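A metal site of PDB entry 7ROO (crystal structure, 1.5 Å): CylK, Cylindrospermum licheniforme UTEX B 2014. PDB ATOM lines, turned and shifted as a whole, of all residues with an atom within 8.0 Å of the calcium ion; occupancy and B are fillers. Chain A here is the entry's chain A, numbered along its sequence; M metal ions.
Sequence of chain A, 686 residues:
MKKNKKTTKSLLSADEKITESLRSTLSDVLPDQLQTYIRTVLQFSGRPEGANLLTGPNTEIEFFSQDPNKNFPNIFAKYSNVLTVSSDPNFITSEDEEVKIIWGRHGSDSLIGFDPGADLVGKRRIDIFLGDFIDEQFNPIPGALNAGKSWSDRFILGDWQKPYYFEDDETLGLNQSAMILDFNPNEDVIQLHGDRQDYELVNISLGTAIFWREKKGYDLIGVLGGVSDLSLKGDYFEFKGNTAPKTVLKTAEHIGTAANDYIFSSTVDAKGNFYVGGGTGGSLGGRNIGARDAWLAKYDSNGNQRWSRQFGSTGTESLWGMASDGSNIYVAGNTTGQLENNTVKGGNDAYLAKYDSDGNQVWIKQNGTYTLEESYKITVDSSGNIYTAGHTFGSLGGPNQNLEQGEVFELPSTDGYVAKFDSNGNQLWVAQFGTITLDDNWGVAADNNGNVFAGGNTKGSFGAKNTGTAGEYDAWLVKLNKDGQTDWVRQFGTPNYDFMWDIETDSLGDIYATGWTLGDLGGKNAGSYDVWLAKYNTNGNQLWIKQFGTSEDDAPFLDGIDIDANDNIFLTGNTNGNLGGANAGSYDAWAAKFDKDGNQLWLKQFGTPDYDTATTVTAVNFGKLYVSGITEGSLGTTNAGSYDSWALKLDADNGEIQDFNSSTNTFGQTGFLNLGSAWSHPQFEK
The calcium ion is bound by O of Thr 608 (2.3 Å), OD2 of Asp 612 (2.3 Å), OD1 of Asp 588 (2.3 Å), O of Gly 585 (2.3 Å), O of Asp 610 (2.4 Å) and O of Tyr 587 (2.4 Å).
The side-chain hydroxyl (OG1) of Thr 608 lies within hydrogen-bond range of the backbone NH (N) of Asp 610, at 2.9 Å. OD1 of Asp 612 sits at hydrogen-bond distance from OG1 of Thr 631. The side-chain carboxylate of Asp 588 lies within hydrogen-bond range of the backbone NH of Ala 584, at 2.8 Å. N of Asp 588 is in hydrogen-bond range of O of Thr 575. The side-chain carboxylate (OD2) of Asp 588 lies within hydrogen-bond range of the side-chain amide nitrogen (NE2) of Gln 605 (3.0 Å). OD1 of Asn 583 sits at hydrogen-bond distance from N of Gly 585 (2.7 Å). The side-chain hydroxyl of Tyr 587 lies within hydrogen-bond range of the side-chain amide nitrogen of Asn 576, at 3.4 Å.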
ATOM      1  N   THR A 575     -31.321   1.215  29.714  1.00  0.00           N
ATOM      2  CA  THR A 575     -30.648   1.574  30.983  1.00  0.00           C
ATOM      3  C   THR A 575     -29.259   2.076  30.636  1.00  0.00           C
ATOM      4  O   THR A 575     -28.600   1.473  29.729  1.00  0.00           O
ATOM      5  CB  THR A 575     -30.577   0.369  31.917  1.00  0.00           C
ATOM      6  OG1 THR A 575     -29.929   0.776  33.132  1.00  0.00           O
ATOM      7  CG2 THR A 575     -29.797  -0.805  31.331  1.00  0.00           C
ATOM      8  N   ASN A 576     -28.767   3.031  31.402  1.00  0.00           N
ATOM      9  CA  ASN A 576     -27.345   3.418  31.333  1.00  0.00           C
ATOM     10  C   ASN A 576     -26.655   2.963  32.625  1.00  0.00           C
ATOM     11  O   ASN A 576     -25.568   3.431  32.859  1.00  0.00           O
ATOM     12  CB  ASN A 576     -27.072   4.890  31.043  1.00  0.00           C
ATOM     13  CG  ASN A 576     -27.538   5.839  32.114  1.00  0.00           C
ATOM     14  OD1 ASN A 576     -28.137   5.422  33.085  1.00  0.00           O
ATOM     15  ND2 ASN A 576     -27.274   7.121  31.909  1.00  0.00           N
ATOM     16  N   ASN A 583     -22.769  -2.909  31.973  1.00  0.00           N
ATOM     17  CA  ASN A 583     -23.162  -1.993  30.867  1.00  0.00           C
ATOM     18  C   ASN A 583     -22.052  -2.005  29.800  1.00  0.00           C
ATOM     19  O   ASN A 583     -20.871  -1.884  30.145  1.00  0.00           O
ATOM     20  CB  ASN A 583     -23.479  -0.623  31.426  1.00  0.00           C
ATOM     21  CG  ASN A 583     -24.002   0.317  30.367  1.00  0.00           C
ATOM     22  OD1 ASN A 583     -23.222   0.748  29.497  1.00  0.00           O
ATOM     23  ND2 ASN A 583     -25.297   0.587  30.459  1.00  0.00           N
ATOM     24  N   ALA A 584     -22.423  -2.174  28.537  1.00  0.00           N
ATOM     25  CA  ALA A 584     -21.493  -2.247  27.388  1.00  0.00           C
ATOM     26  C   ALA A 584     -21.034  -0.849  26.969  1.00  0.00           C
ATOM     27  O   ALA A 584     -19.965  -0.725  26.340  1.00  0.00           O
ATOM     28  CB  ALA A 584     -22.145  -2.937  26.219  1.00  0.00           C
ATOM     29  N   GLY A 585     -21.752   0.206  27.358  1.00  0.00           N
ATOM     30  CA  GLY A 585     -21.411   1.586  26.984  1.00  0.00           C
ATOM     31  C   GLY A 585     -22.712   2.378  26.708  1.00  0.00           C
ATOM     32  O   GLY A 585     -23.633   1.808  26.097  1.00  0.00           O
ATOM     33  N   SER A 586     -22.779   3.640  27.149  1.00  0.00           N
ATOM     34  CA  SER A 586     -23.965   4.507  26.907  1.00  0.00           C
ATOM     35  C   SER A 586     -25.189   3.808  27.525  1.00  0.00           C
ATOM     36  O   SER A 586     -25.066   3.138  28.606  1.00  0.00           O
ATOM     37  CB  SER A 586     -24.052   4.769  25.454  1.00  0.00           C
ATOM     38  OG  SER A 586     -25.075   5.709  25.125  1.00  0.00           O
ATOM     39  N   TYR A 587     -26.347   3.955  26.857  1.00  0.00           N
ATOM     40  CA  TYR A 587     -27.550   3.161  27.152  1.00  0.00           C
ATOM     41  C   TYR A 587     -27.414   1.813  26.450  1.00  0.00           C
ATOM     42  O   TYR A 587     -26.821   1.737  25.339  1.00  0.00           O
ATOM     43  CB  TYR A 587     -28.808   3.912  26.709  1.00  0.00           C
ATOM     44  CG  TYR A 587     -29.090   5.119  27.607  1.00  0.00           C
ATOM     45  CD1 TYR A 587     -28.394   6.315  27.478  1.00  0.00           C
ATOM     46  CD2 TYR A 587     -30.048   5.018  28.588  1.00  0.00           C
ATOM     47  CE1 TYR A 587     -28.663   7.403  28.301  1.00  0.00           C
ATOM     48  CE2 TYR A 587     -30.345   6.099  29.404  1.00  0.00           C
ATOM     49  CZ  TYR A 587     -29.612   7.275  29.273  1.00  0.00           C
ATOM     50  OH  TYR A 587     -29.823   8.402  30.046  1.00  0.00           O
ATOM     51  N   ASP A 588     -27.898   0.796  27.125  1.00  0.00           N
ATOM     52  CA  ASP A 588     -28.065  -0.565  26.588  1.00  0.00           C
ATOM     53  C   ASP A 588     -29.548  -0.940  26.589  1.00  0.00           C
ATOM     54  O   ASP A 588     -30.329  -0.326  27.366  1.00  0.00           O
ATOM     55  CB  ASP A 588     -27.347  -1.615  27.431  1.00  0.00           C
ATOM     56  CG  ASP A 588     -25.838  -1.637  27.371  1.00  0.00           C
ATOM     57  OD1 ASP A 588     -25.262  -1.027  26.451  1.00  0.00           O
ATOM     58  OD2 ASP A 588     -25.250  -2.336  28.275  1.00  0.00           O
ATOM     59  N   ALA A 589     -29.948  -1.968  25.873  1.00  0.00           N
ATOM     60  CA  ALA A 589     -31.283  -2.584  25.974  1.00  0.00           C
ATOM     61  C   ALA A 589     -31.354  -3.482  27.194  1.00  0.00           C
ATOM     62  O   ALA A 589     -30.299  -3.955  27.653  1.00  0.00           O
ATOM     63  CB  ALA A 589     -31.572  -3.387  24.754  1.00  0.00           C
ATOM     64  N   GLN A 605     -29.611  -7.974  30.023  1.00  0.00           N
ATOM     65  CA  GLN A 605     -29.153  -6.685  29.458  1.00  0.00           C
ATOM     66  C   GLN A 605     -28.218  -6.987  28.286  1.00  0.00           C
ATOM     67  O   GLN A 605     -27.417  -7.916  28.388  1.00  0.00           O
ATOM     68  CB  GLN A 605     -28.452  -5.849  30.525  1.00  0.00           C
ATOM     69  CG  GLN A 605     -27.875  -4.524  30.043  1.00  0.00           C
ATOM     70  CD  GLN A 605     -27.517  -3.585  31.167  1.00  0.00           C
ATOM     71  OE1 GLN A 605     -28.085  -3.715  32.248  1.00  0.00           O
ATOM     72  NE2 GLN A 605     -26.616  -2.620  30.895  1.00  0.00           N
ATOM     73  N   PHE A 606     -28.306  -6.223  27.221  1.00  0.00           N
ATOM     74  CA  PHE A 606     -27.548  -6.520  25.997  1.00  0.00           C
ATOM     75  C   PHE A 606     -27.410  -5.236  25.187  1.00  0.00           C
ATOM     76  O   PHE A 606     -28.257  -4.322  25.298  1.00  0.00           O
ATOM     77  CB  PHE A 606     -28.212  -7.643  25.201  1.00  0.00           C
ATOM     78  CG  PHE A 606     -29.707  -7.615  25.162  1.00  0.00           C
ATOM     79  CD1 PHE A 606     -30.418  -8.290  26.133  1.00  0.00           C
ATOM     80  CD2 PHE A 606     -30.414  -6.952  24.175  1.00  0.00           C
ATOM     81  CE1 PHE A 606     -31.799  -8.323  26.145  1.00  0.00           C
ATOM     82  CE2 PHE A 606     -31.805  -7.003  24.172  1.00  0.00           C
ATOM     83  CZ  PHE A 606     -32.491  -7.647  25.165  1.00  0.00           C
ATOM     84  N   GLY A 607     -26.324  -5.130  24.458  1.00  0.00           N
ATOM     85  CA  GLY A 607     -26.161  -4.027  23.513  1.00  0.00           C
ATOM     86  C   GLY A 607     -24.740  -3.846  23.053  1.00  0.00           C
ATOM     87  O   GLY A 607     -23.935  -4.811  23.147  1.00  0.00           O
ATOM     88  N   THR A 608     -24.428  -2.674  22.580  1.00  0.00           N
ATOM     89  CA  THR A 608     -23.127  -2.312  21.975  1.00  0.00           C
ATOM     90  C   THR A 608     -22.485  -1.270  22.882  1.00  0.00           C
ATOM     91  O   THR A 608     -23.165  -0.689  23.768  1.00  0.00           O
ATOM     92  CB  THR A 608     -23.292  -1.737  20.573  1.00  0.00           C
ATOM     93  OG1 THR A 608     -23.699  -0.378  20.724  1.00  0.00           O
ATOM     94  CG2 THR A 608     -24.209  -2.496  19.664  1.00  0.00           C
ATOM     95  N   PRO A 609     -21.192  -0.937  22.730  1.00  0.00           N
ATOM     96  CA  PRO A 609     -20.574   0.203  23.400  1.00  0.00           C
ATOM     97  C   PRO A 609     -21.247   1.556  23.106  1.00  0.00           C
ATOM     98  O   PRO A 609     -20.951   2.562  23.760  1.00  0.00           O
ATOM     99  CB  PRO A 609     -19.135   0.138  22.895  1.00  0.00           C
ATOM    100  CG  PRO A 609     -18.929  -1.326  22.583  1.00  0.00           C
ATOM    101  CD  PRO A 609     -20.237  -1.700  21.913  1.00  0.00           C
ATOM    102  N   ASP A 610     -22.057   1.628  22.064  1.00  0.00           N
ATOM    103  CA  ASP A 610     -22.719   2.876  21.658  1.00  0.00           C
ATOM    104  C   ASP A 610     -24.143   2.874  22.232  1.00  0.00           C
ATOM    105  O   ASP A 610     -24.537   1.935  22.907  1.00  0.00           O
ATOM    106  CB  ASP A 610     -22.717   3.024  20.135  1.00  0.00           C
ATOM    107  CG  ASP A 610     -21.445   3.627  19.597  1.00  0.00           C
ATOM    108  OD1 ASP A 610     -21.280   4.850  19.782  1.00  0.00           O
ATOM    109  OD2 ASP A 610     -20.697   2.915  18.888  1.00  0.00           O
ATOM    110  N   TYR A 611     -24.902   3.889  21.912  1.00  0.00           N
ATOM    111  CA  TYR A 611     -26.309   4.017  22.391  1.00  0.00           C
ATOM    112  C   TYR A 611     -27.131   2.859  21.832  1.00  0.00           C
ATOM    113  O   TYR A 611     -27.241   2.743  20.570  1.00  0.00           O
ATOM    114  CB  TYR A 611     -26.881   5.376  21.959  1.00  0.00           C
ATOM    115  CG  TYR A 611     -28.293   5.541  22.446  1.00  0.00           C
ATOM    116  CD1 TYR A 611     -29.383   5.132  21.698  1.00  0.00           C
ATOM    117  CD2 TYR A 611     -28.562   6.110  23.659  1.00  0.00           C
ATOM    118  CE1 TYR A 611     -30.676   5.187  22.206  1.00  0.00           C
ATOM    119  CE2 TYR A 611     -29.829   6.196  24.175  1.00  0.00           C
ATOM    120  CZ  TYR A 611     -30.909   5.793  23.419  1.00  0.00           C
ATOM    121  OH  TYR A 611     -32.174   5.821  23.961  1.00  0.00           O
ATOM    122  N   ASP A 612     -27.895   2.159  22.676  1.00  0.00           N
ATOM    123  CA  ASP A 612     -28.923   1.187  22.251  1.00  0.00           C
ATOM    124  C   ASP A 612     -30.179   1.384  23.110  1.00  0.00           C
ATOM    125  O   ASP A 612     -30.061   1.701  24.323  1.00  0.00           O
ATOM    126  CB  ASP A 612     -28.475  -0.258  22.400  1.00  0.00           C
ATOM    127  CG  ASP A 612     -26.996  -0.433  22.257  1.00  0.00           C
ATOM    128  OD1 ASP A 612     -26.469  -0.358  21.097  1.00  0.00           O
ATOM    129  OD2 ASP A 612     -26.359  -0.697  23.346  1.00  0.00           O
ATOM    130  N   THR A 613     -31.346   1.114  22.539  1.00  0.00           N
ATOM    131  CA  THR A 613     -32.556   0.902  23.360  1.00  0.00           C
ATOM    132  C   THR A 613     -33.435  -0.144  22.722  1.00  0.00           C
ATOM    133  O   THR A 613     -33.580  -0.116  21.481  1.00  0.00           O
ATOM    134  CB  THR A 613     -33.336   2.196  23.654  1.00  0.00           C
ATOM    135  OG1 THR A 613     -34.461   1.871  24.496  1.00  0.00           O
ATOM    136  CG2 THR A 613     -33.871   2.875  22.408  1.00  0.00           C
ATOM    137  N   ILE A 630     -33.315  -0.257  18.544  1.00  0.00           N
ATOM    138  CA  ILE A 630     -32.460   0.654  17.754  1.00  0.00           C
ATOM    139  C   ILE A 630     -31.090   0.804  18.364  1.00  0.00           C
ATOM    140  O   ILE A 630     -30.866   0.509  19.549  1.00  0.00           O
ATOM    141  CB  ILE A 630     -33.187   1.989  17.546  1.00  0.00           C
ATOM    142  CG1 ILE A 630     -33.282   2.768  18.868  1.00  0.00           C
ATOM    143  CG2 ILE A 630     -34.535   1.703  16.916  1.00  0.00           C
ATOM    144  CD1 ILE A 630     -33.979   4.119  18.758  1.00  0.00           C
ATOM    145  N   THR A 631     -30.144   1.214  17.531  1.00  0.00           N
ATOM    146  CA  THR A 631     -28.748   1.353  17.976  1.00  0.00           C
ATOM    147  C   THR A 631     -27.957   2.346  17.114  1.00  0.00           C
ATOM    148  O   THR A 631     -28.276   2.511  15.891  1.00  0.00           O
ATOM    149  CB  THR A 631     -28.070  -0.017  17.902  1.00  0.00           C
ATOM    150  OG1 THR A 631     -26.781   0.131  18.513  1.00  0.00           O
ATOM    151  CG2 THR A 631     -27.874  -0.554  16.508  1.00  0.00           C
ATOM    152  N   GLU A 632     -26.956   2.976  17.725  1.00  0.00           N
ATOM    153  CA  GLU A 632     -25.933   3.762  16.989  1.00  0.00           C
ATOM    154  C   GLU A 632     -24.688   2.887  16.740  1.00  0.00           C
ATOM    155  O   GLU A 632     -23.746   3.374  16.102  1.00  0.00           O
ATOM    156  CB  GLU A 632     -25.548   5.023  17.799  1.00  0.00           C
ATOM    157  CG  GLU A 632     -26.699   5.999  17.907  1.00  0.00           C
ATOM    158  CD  GLU A 632     -26.383   7.169  18.794  1.00  0.00           C
ATOM    159  OE1 GLU A 632     -25.211   7.609  18.783  1.00  0.00           O
ATOM    160  OE2 GLU A 632     -27.276   7.652  19.533  1.00  0.00           O
ATOM    161  N   GLY A 633     -24.683   1.670  17.287  1.00  0.00           N
ATOM    162  CA  GLY A 633     -23.525   0.795  17.062  1.00  0.00           C
ATOM    163  C   GLY A 633     -23.749  -0.262  16.000  1.00  0.00           C
ATOM    164  O   GLY A 633     -24.659  -0.130  15.176  1.00  0.00           O
ATOM    165  N   LEU A 635     -24.854  -3.827  15.730  1.00  0.00           N
ATOM    166  CA  LEU A 635     -25.540  -4.884  16.459  1.00  0.00           C
ATOM    167  C   LEU A 635     -26.139  -5.832  15.413  1.00  0.00           C
ATOM    168  O   LEU A 635     -27.040  -5.445  14.612  1.00  0.00           O
ATOM    169  CB  LEU A 635     -26.546  -4.290  17.425  1.00  0.00           C
ATOM    170  CG  LEU A 635     -26.959  -5.163  18.614  1.00  0.00           C
ATOM    171  CD1 LEU A 635     -27.760  -4.340  19.640  1.00  0.00           C
ATOM    172  CD2 LEU A 635     -27.759  -6.381  18.179  1.00  0.00           C
HETATM  173 CA    CA M   1     -24.916   0.451  24.715  1.00  0.00          CA
